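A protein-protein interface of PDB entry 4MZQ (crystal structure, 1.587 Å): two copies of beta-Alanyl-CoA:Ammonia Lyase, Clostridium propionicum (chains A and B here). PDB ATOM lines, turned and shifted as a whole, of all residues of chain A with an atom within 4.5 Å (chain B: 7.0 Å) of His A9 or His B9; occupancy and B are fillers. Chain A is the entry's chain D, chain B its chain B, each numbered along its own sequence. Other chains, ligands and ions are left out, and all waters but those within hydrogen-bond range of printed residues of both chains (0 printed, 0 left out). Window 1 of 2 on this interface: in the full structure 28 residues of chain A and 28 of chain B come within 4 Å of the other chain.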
ATOM      1  N   VAL A   7      30.630  29.646  29.827  1.00  0.00           N
ATOM      2  CA  VAL A   7      29.745  29.864  28.697  1.00  0.00           C
ATOM      3  C   VAL A   7      28.947  28.599  28.399  1.00  0.00           C
ATOM      4  O   VAL A   7      29.507  27.591  27.973  1.00  0.00           O
ATOM      5  CB  VAL A   7      30.542  30.284  27.445  1.00  0.00           C
ATOM      6  CG1 VAL A   7      29.639  30.398  26.218  1.00  0.00           C
ATOM      7  CG2 VAL A   7      31.293  31.610  27.710  1.00  0.00           C
ATOM      8  N   HIS A   8      27.645  28.628  28.657  1.00  0.00           N
ATOM      9  CA  HIS A   8      26.792  27.578  28.127  1.00  0.00           C
ATOM     10  C   HIS A   8      26.282  28.007  26.765  1.00  0.00           C
ATOM     11  O   HIS A   8      26.208  29.194  26.473  1.00  0.00           O
ATOM     12  CB  HIS A   8      25.633  27.264  29.079  1.00  0.00           C
ATOM     13  CG  HIS A   8      26.054  26.597  30.346  1.00  0.00           C
ATOM     14  ND1 HIS A   8      25.171  25.935  31.175  1.00  0.00           N
ATOM     15  CD2 HIS A   8      27.273  26.480  30.937  1.00  0.00           C
ATOM     16  CE1 HIS A   8      25.820  25.449  32.213  1.00  0.00           C
ATOM     17  NE2 HIS A   8      27.100  25.767  32.092  1.00  0.00           N
ATOM     18  N   HIS A   9      25.956  27.031  25.928  1.00  0.00           N
ATOM     19  CA  HIS A   9      25.584  27.288  24.544  1.00  0.00           C
ATOM     20  C   HIS A   9      24.719  26.130  24.084  1.00  0.00           C
ATOM     21  O   HIS A   9      25.139  24.978  24.176  1.00  0.00           O
ATOM     22  CB  HIS A   9      26.850  27.423  23.675  1.00  0.00           C
ATOM     23  CG  HIS A   9      26.588  27.717  22.231  1.00  0.00           C
ATOM     24  ND1 HIS A   9      27.136  28.806  21.589  1.00  0.00           N
ATOM     25  CD2 HIS A   9      25.872  27.050  21.293  1.00  0.00           C
ATOM     26  CE1 HIS A   9      26.758  28.804  20.322  1.00  0.00           C
ATOM     27  NE2 HIS A   9      25.987  27.753  20.120  1.00  0.00           N
ATOM     28  N   LEU A  10      23.516  26.421  23.596  1.00  0.00           N
ATOM     29  CA  LEU A  10      22.640  25.349  23.134  1.00  0.00           C
ATOM     30  C   LEU A  10      21.542  25.921  22.243  1.00  0.00           C
ATOM     31  O   LEU A  10      21.552  27.112  21.940  1.00  0.00           O
ATOM     32  CB  LEU A  10      22.052  24.573  24.335  1.00  0.00           C
ATOM     33  CG  LEU A  10      21.521  25.363  25.541  1.00  0.00           C
ATOM     34  CD1 LEU A  10      20.282  26.139  25.170  1.00  0.00           C
ATOM     35  CD2 LEU A  10      21.218  24.456  26.719  1.00  0.00           C
ATOM     36  N   GLU A  39      28.144  25.470  37.829  1.00  0.00           N
ATOM     37  CA  GLU A  39      29.465  25.178  37.285  1.00  0.00           C
ATOM     38  C   GLU A  39      30.537  26.082  37.898  1.00  0.00           C
ATOM     39  O   GLU A  39      31.627  25.611  38.257  1.00  0.00           O
ATOM     40  CB  GLU A  39      29.462  25.306  35.762  1.00  0.00           C
ATOM     41  CG  GLU A  39      30.607  24.539  35.132  1.00  0.00           C
ATOM     42  CD  GLU A  39      30.632  24.608  33.625  1.00  0.00           C
ATOM     43  OE1 GLU A  39      29.583  24.854  33.017  1.00  0.00           O
ATOM     44  OE2 GLU A  39      31.711  24.410  33.042  1.00  0.00           O
ATOM     45  N   MET A  69      21.291  30.002  21.631  1.00  0.00           N
ATOM     46  CA  MET A  69      21.504  30.872  22.784  1.00  0.00           C
ATOM     47  C   MET A  69      22.813  30.577  23.508  1.00  0.00           C
ATOM     48  O   MET A  69      23.228  29.406  23.642  1.00  0.00           O
ATOM     49  CB  MET A  69      20.350  30.710  23.782  1.00  0.00           C
ATOM     50  CG  MET A  69      18.989  31.069  23.239  1.00  0.00           C
ATOM     51  SD  MET A  69      18.819  32.829  22.930  1.00  0.00           S
ATOM     52  CE  MET A  69      18.935  33.471  24.603  1.00  0.00           C
ATOM     53  N   GLU A  70      23.454  31.640  23.994  1.00  0.00           N
ATOM     54  CA  GLU A  70      24.600  31.500  24.884  1.00  0.00           C
ATOM     55  C   GLU A  70      24.281  32.109  26.223  1.00  0.00           C
ATOM     56  O   GLU A  70      23.606  33.127  26.301  1.00  0.00           O
ATOM     57  CB  GLU A  70      25.842  32.171  24.319  1.00  0.00           C
ATOM     58  CG  GLU A  70      26.394  31.485  23.131  1.00  0.00           C
ATOM     59  CD  GLU A  70      27.878  31.773  22.926  1.00  0.00           C
ATOM     60  OE1 GLU A  70      28.502  31.067  22.120  1.00  0.00           O
ATOM     61  OE2 GLU A  70      28.417  32.699  23.565  1.00  0.00           O
ATOM     62  N   VAL A  92      22.504  34.051  19.258  1.00  0.00           N
ATOM     63  CA  VAL A  92      23.576  34.003  18.268  1.00  0.00           C
ATOM     64  C   VAL A  92      23.076  33.520  16.905  1.00  0.00           C
ATOM     65  O   VAL A  92      23.761  33.678  15.903  1.00  0.00           O
ATOM     66  CB  VAL A  92      24.740  33.109  18.757  1.00  0.00           C
ATOM     67  CG1 VAL A  92      25.236  33.620  20.095  1.00  0.00           C
ATOM     68  CG2 VAL A  92      24.312  31.660  18.886  1.00  0.00           C
ATOM     69  N   LYS B   4      34.224  27.670  11.487  1.00  0.00           N
ATOM     70  CA  LYS B   4      34.724  27.536  12.847  1.00  0.00           C
ATOM     71  C   LYS B   4      34.083  26.324  13.496  1.00  0.00           C
ATOM     72  O   LYS B   4      33.057  25.850  13.031  1.00  0.00           O
ATOM     73  CB  LYS B   4      34.427  28.796  13.669  1.00  0.00           C
ATOM     74  CG  LYS B   4      32.956  28.955  14.067  1.00  0.00           C
ATOM     75  CD  LYS B   4      32.698  30.285  14.785  1.00  0.00           C
ATOM     76  CE  LYS B   4      31.259  30.379  15.268  1.00  0.00           C
ATOM     77  NZ  LYS B   4      30.944  31.665  15.944  1.00  0.00           N
ATOM     78  N   VAL B   6      31.806  24.620  16.182  1.00  0.00           N
ATOM     79  CA  VAL B   6      30.693  25.022  17.039  1.00  0.00           C
ATOM     80  C   VAL B   6      30.736  24.210  18.330  1.00  0.00           C
ATOM     81  O   VAL B   6      30.952  22.996  18.316  1.00  0.00           O
ATOM     82  CB  VAL B   6      29.341  24.855  16.318  1.00  0.00           C
ATOM     83  CG1 VAL B   6      28.186  24.871  17.307  1.00  0.00           C
ATOM     84  CG2 VAL B   6      29.173  25.960  15.285  1.00  0.00           C
ATOM     85  N   VAL B   7      30.593  24.901  19.452  1.00  0.00           N
ATOM     86  CA  VAL B   7      30.677  24.261  20.752  1.00  0.00           C
ATOM     87  C   VAL B   7      29.398  24.494  21.534  1.00  0.00           C
ATOM     88  O   VAL B   7      29.084  25.625  21.888  1.00  0.00           O
ATOM     89  CB  VAL B   7      31.868  24.796  21.576  1.00  0.00           C
ATOM     90  CG1 VAL B   7      31.860  24.203  22.973  1.00  0.00           C
ATOM     91  CG2 VAL B   7      33.165  24.490  20.879  1.00  0.00           C
ATOM     92  N   HIS B   8      28.647  23.428  21.780  1.00  0.00           N
ATOM     93  CA  HIS B   8      27.569  23.496  22.754  1.00  0.00           C
ATOM     94  C   HIS B   8      28.110  23.076  24.123  1.00  0.00           C
ATOM     95  O   HIS B   8      29.062  22.312  24.214  1.00  0.00           O
ATOM     96  CB  HIS B   8      26.383  22.619  22.333  1.00  0.00           C
ATOM     97  CG  HIS B   8      25.661  23.125  21.121  1.00  0.00           C
ATOM     98  ND1 HIS B   8      24.388  22.717  20.780  1.00  0.00           N
ATOM     99  CD2 HIS B   8      26.036  24.018  20.171  1.00  0.00           C
ATOM    100  CE1 HIS B   8      24.011  23.332  19.674  1.00  0.00           C
ATOM    101  NE2 HIS B   8      24.997  24.118  19.277  1.00  0.00           N
ATOM    102  N   HIS B   9      27.501  23.585  25.186  1.00  0.00           N
ATOM    103  CA  HIS B   9      28.035  23.381  26.534  1.00  0.00           C
ATOM    104  C   HIS B   9      26.858  23.517  27.480  1.00  0.00           C
ATOM    105  O   HIS B   9      26.156  24.522  27.451  1.00  0.00           O
ATOM    106  CB  HIS B   9      29.147  24.401  26.837  1.00  0.00           C
ATOM    107  CG  HIS B   9      29.721  24.309  28.220  1.00  0.00           C
ATOM    108  ND1 HIS B   9      31.081  24.248  28.454  1.00  0.00           N
ATOM    109  CD2 HIS B   9      29.133  24.335  29.442  1.00  0.00           C
ATOM    110  CE1 HIS B   9      31.300  24.207  29.756  1.00  0.00           C
ATOM    111  NE2 HIS B   9      30.134  24.261  30.379  1.00  0.00           N
ATOM    112  N   LEU B  10      26.609  22.481  28.270  1.00  0.00           N
ATOM    113  CA  LEU B  10      25.475  22.491  29.178  1.00  0.00           C
ATOM    114  C   LEU B  10      25.652  21.442  30.274  1.00  0.00           C
ATOM    115  O   LEU B  10      26.688  20.769  30.329  1.00  0.00           O
ATOM    116  CB  LEU B  10      24.168  22.251  28.406  1.00  0.00           C
ATOM    117  CG  LEU B  10      24.142  21.125  27.370  1.00  0.00           C
ATOM    118  CD1 LEU B  10      24.119  19.770  28.015  1.00  0.00           C
ATOM    119  CD2 LEU B  10      22.966  21.267  26.419  1.00  0.00           C
ATOM    120  N   MET B  11      24.639  21.307  31.131  1.00  0.00           N
ATOM    121  CA  MET B  11      24.700  20.376  32.260  1.00  0.00           C
ATOM    122  C   MET B  11      23.740  19.213  32.069  1.00  0.00           C
ATOM    123  O   MET B  11      22.635  19.397  31.561  1.00  0.00           O
ATOM    124  CB  MET B  11      24.355  21.097  33.564  1.00  0.00           C
ATOM    125  CG  MET B  11      24.603  20.258  34.814  1.00  0.00           C
ATOM    126  SD  MET B  11      24.004  21.076  36.288  1.00  0.00           S
ATOM    127  CE  MET B  11      22.283  20.554  36.291  1.00  0.00           C
ATOM    128  N   GLN B  32      22.167  16.240  20.991  1.00  0.00           N
ATOM    129  CA  GLN B  32      22.937  17.482  20.978  1.00  0.00           C
ATOM    130  C   GLN B  32      23.697  17.689  19.676  1.00  0.00           C
ATOM    131  O   GLN B  32      23.734  18.808  19.149  1.00  0.00           O
ATOM    132  CB  GLN B  32      23.914  17.538  22.156  1.00  0.00           C
ATOM    133  CG  GLN B  32      24.211  18.963  22.586  1.00  0.00           C
ATOM    134  CD  GLN B  32      22.950  19.708  23.000  1.00  0.00           C
ATOM    135  OE1 GLN B  32      22.111  19.170  23.731  1.00  0.00           O
ATOM    136  NE2 GLN B  32      22.797  20.941  22.520  1.00  0.00           N
ATOM    137  N   VAL B  36      23.960  20.761  17.080  1.00  0.00           N
ATOM    138  CA  VAL B  36      25.256  21.312  16.666  1.00  0.00           C
ATOM    139  C   VAL B  36      25.314  21.351  15.144  1.00  0.00           C
ATOM    140  O   VAL B  36      25.726  22.363  14.549  1.00  0.00           O
ATOM    141  CB  VAL B  36      26.435  20.490  17.228  1.00  0.00           C
ATOM    142  CG1 VAL B  36      27.757  20.905  16.566  1.00  0.00           C
ATOM    143  CG2 VAL B  36      26.546  20.679  18.739  1.00  0.00           C
ATOM    144  N   GLU B  39      23.222  24.137  13.766  1.00  0.00           N
ATOM    145  CA  GLU B  39      23.863  25.458  13.875  1.00  0.00           C
ATOM    146  C   GLU B  39      24.896  25.675  12.759  1.00  0.00           C
ATOM    147  O   GLU B  39      24.963  26.757  12.152  1.00  0.00           O
ATOM    148  CB  GLU B  39      24.512  25.632  15.255  1.00  0.00           C
ATOM    149  CG  GLU B  39      24.923  27.073  15.520  1.00  0.00           C
ATOM    150  CD  GLU B  39      25.418  27.328  16.924  1.00  0.00           C
ATOM    151  OE1 GLU B  39      25.244  26.465  17.798  1.00  0.00           O
ATOM    152  OE2 GLU B  39      25.996  28.411  17.157  1.00  0.00           O
ATOM    153  N   TYR B  43      24.925  28.580   9.703  1.00  0.00           N
ATOM    154  CA  TYR B  43      26.047  29.457   9.397  1.00  0.00           C
ATOM    155  C   TYR B  43      26.599  29.293   7.978  1.00  0.00           C
ATOM    156  O   TYR B  43      27.012  30.281   7.354  1.00  0.00           O
ATOM    157  CB  TYR B  43      27.171  29.236  10.411  1.00  0.00           C
ATOM    158  CG  TYR B  43      26.795  29.586  11.834  1.00  0.00           C
ATOM    159  CD1 TYR B  43      25.779  30.493  12.111  1.00  0.00           C
ATOM    160  CD2 TYR B  43      27.468  29.017  12.900  1.00  0.00           C
ATOM    161  CE1 TYR B  43      25.443  30.812  13.410  1.00  0.00           C
ATOM    162  CE2 TYR B  43      27.134  29.328  14.208  1.00  0.00           C
ATOM    163  CZ  TYR B  43      26.125  30.227  14.458  1.00  0.00           C
ATOM    164  OH  TYR B  43      25.781  30.545  15.756  1.00  0.00           O
ATOM    165  N   PHE B  68      28.917  17.983  33.563  1.00  0.00           N
ATOM    166  CA  PHE B  68      28.863  19.089  32.617  1.00  0.00           C
ATOM    167  C   PHE B  68      29.531  18.654  31.317  1.00  0.00           C
ATOM    168  O   PHE B  68      30.591  18.034  31.333  1.00  0.00           O
ATOM    169  CB  PHE B  68      29.522  20.338  33.198  1.00  0.00           C
ATOM    170  CG  PHE B  68      28.714  21.001  34.282  1.00  0.00           C
ATOM    171  CD1 PHE B  68      28.775  20.541  35.591  1.00  0.00           C
ATOM    172  CD2 PHE B  68      27.900  22.091  33.998  1.00  0.00           C
ATOM    173  CE1 PHE B  68      28.039  21.154  36.593  1.00  0.00           C
ATOM    174  CE2 PHE B  68      27.181  22.714  34.995  1.00  0.00           C
ATOM    175  CZ  PHE B  68      27.241  22.247  36.292  1.00  0.00           C
ATOM    176  N   MET B  69      28.887  18.950  30.190  1.00  0.00           N
ATOM    177  CA  MET B  69      29.279  18.362  28.915  1.00  0.00           C
ATOM    178  C   MET B  69      29.444  19.387  27.817  1.00  0.00           C
ATOM    179  O   MET B  69      28.675  20.355  27.717  1.00  0.00           O
ATOM    180  CB  MET B  69      28.242  17.336  28.450  1.00  0.00           C
ATOM    181  CG  MET B  69      28.032  16.179  29.408  1.00  0.00           C
ATOM    182  SD  MET B  69      29.403  15.009  29.357  1.00  0.00           S
ATOM    183  CE  MET B  69      29.254  14.381  27.688  1.00  0.00           C
ATOM    184  N   GLU B  70      30.423  19.144  26.965  1.00  0.00           N
ATOM    185  CA  GLU B  70      30.556  19.924  25.757  1.00  0.00           C
ATOM    186  C   GLU B  70      30.372  19.034  24.548  1.00  0.00           C
ATOM    187  O   GLU B  70      30.684  17.833  24.577  1.00  0.00           O
ATOM    188  CB  GLU B  70      31.913  20.621  25.698  1.00  0.00           C
ATOM    189  CG  GLU B  70      32.075  21.685  26.732  1.00  0.00           C
ATOM    190  CD  GLU B  70      33.199  22.627  26.401  1.00  0.00           C
ATOM    191  OE1 GLU B  70      33.228  23.730  26.973  1.00  0.00           O
ATOM    192  OE2 GLU B  70      34.058  22.261  25.567  1.00  0.00           O
ATOM    193  N   TYR B  71      29.863  19.639  23.483  1.00  0.00           N
ATOM    194  CA  TYR B  71      29.594  18.939  22.236  1.00  0.00           C
ATOM    195  C   TYR B  71      30.197  19.793  21.141  1.00  0.00           C
ATOM    196  O   TYR B  71      29.777  20.930  20.929  1.00  0.00           O
ATOM    197  CB  TYR B  71      28.083  18.712  22.037  1.00  0.00           C
ATOM    198  CG  TYR B  71      27.439  18.016  23.227  1.00  0.00           C
ATOM    199  CD1 TYR B  71      27.252  16.634  23.245  1.00  0.00           C
ATOM    200  CD2 TYR B  71      27.077  18.741  24.356  1.00  0.00           C
ATOM    201  CE1 TYR B  71      26.697  16.000  24.354  1.00  0.00           C
ATOM    202  CE2 TYR B  71      26.532  18.125  25.452  1.00  0.00           C
ATOM    203  CZ  TYR B  71      26.327  16.763  25.450  1.00  0.00           C
ATOM    204  OH  TYR B  71      25.772  16.173  26.564  1.00  0.00           O
ATOM    205  N   VAL B  92      33.446  17.843  31.192  1.00  0.00           N
ATOM    206  CA  VAL B  92      34.312  18.874  31.774  1.00  0.00           C
ATOM    207  C   VAL B  92      34.176  19.029  33.291  1.00  0.00           C
ATOM    208  O   VAL B  92      35.034  19.639  33.933  1.00  0.00           O
ATOM    209  CB  VAL B  92      34.059  20.260  31.123  1.00  0.00           C
ATOM    210  CG1 VAL B  92      34.329  20.199  29.636  1.00  0.00           C
ATOM    211  CG2 VAL B  92      32.636  20.737  31.405  1.00  0.00           C
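The backbone carbonyl oxygen (O) of Phe B68 sits at hydrogen-bond distance from the backbone NH (N) of Val B92 (2.9 Å). ND1 of His B9 lies within hydrogen-bond range of OE1 of Glu B70, at 2.7 Å. N of Met B69 lies within hydrogen-bond range of O of Leu B10, 2.9 Å away. The side-chain hydroxyl (OH) of Tyr B43 is in hydrogen-bond range of the side-chain carboxylate (OE2) of Glu B39 (2.6 Å). A ring nitrogen (ND1) of His B8 lies within hydrogen-bond range of the side-chain amide nitrogen (NE2) of Gln B32 (3.0 Å). The side-chain carboxylate of Glu A70 sits at hydrogen-bond distance from a ring nitrogen (ND1) of His A9, at 2.7 Å.
Of chain B, only Val B7, His B8, His B9 and Glu B39 come within 4 Å of His A9. Printed residues of chain B within 4 Å of Leu A10: His B8 (3.9 Å) and Leu B10 (3.6 Å). His B9 touches four residues of chain A. Gln B32 touches none of the printed residues of chain A. Of the printed residues of chain A, Phe B68 touches Glu A39. The nearest printed residue of chain A that does not touch Tyr B43 is His A9 (5.0 Å).
NE2 of His B9 lies within hydrogen-bond range of OE1 of Glu A39, at 2.8 Å. N of His B9 sits at hydrogen-bond distance from O of His A9, 2.9 Å away. OE1 of Glu B39 is in hydrogen-bond range of NE2 of His A9 (2.8 Å).
Among the printed residues, pairs that only touch across the chains: His A9 with His B8 (3.2 Å), His A8 with His B9 (3.2 Å), His A9 with Val B7 (3.3 Å), Val A7 with His B9 (3.3 Å), Glu A39 with Phe B68 (3.4 Å), Val A92 with Tyr B43 (3.6 Å), Leu A10 with Leu B10 (3.6 Å), Leu A10 with His B8 (3.9 Å) and His A8 with Leu B10 (3.99 Å).
Of the 8 printed residues of chain A, 6 touch a printed residue of chain B. Printed residues of chain A that touch a printed residue of chain B: Val A7, His A8, His A9, Leu A10, Glu A39 and Val A92. Hydrophobic or aromatic side chains of chain A that line the printed part of chain B: His A8, His A9, Leu A10 and Val A92. Along chain A the printed residues that touch a printed residue of chain B span positions 7 to 92. Of the 16 printed residues of chain B, 7 touch a printed residue of chain A. Hydrophobic or aromatic side chains of chain B within 4 Å of the printed part of chain A: His B8, His B9, Leu B10, Tyr B43 and Phe B68. Among the printed residues, no Asp or Glu carboxylate lies within 4 Å of a Lys or Arg side-chain nitrogen of the other chain.
His A8 touches Leu B10, and with the chains exchanged Leu A10 touches His B8. His B9 touches its own counterpart, His A9. His A9 touches Glu B39, and with the chains exchanged Glu A39 touches His B9. Leu B10 touches its own counterpart, Leu A10. Positions printed for both chains: 7, 8, 9, 10, 39, 69, 70 and 92. Of the 12 pairs that touch across the chains among the printed residues, 10 have their exchanged pair printed and touching as well.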
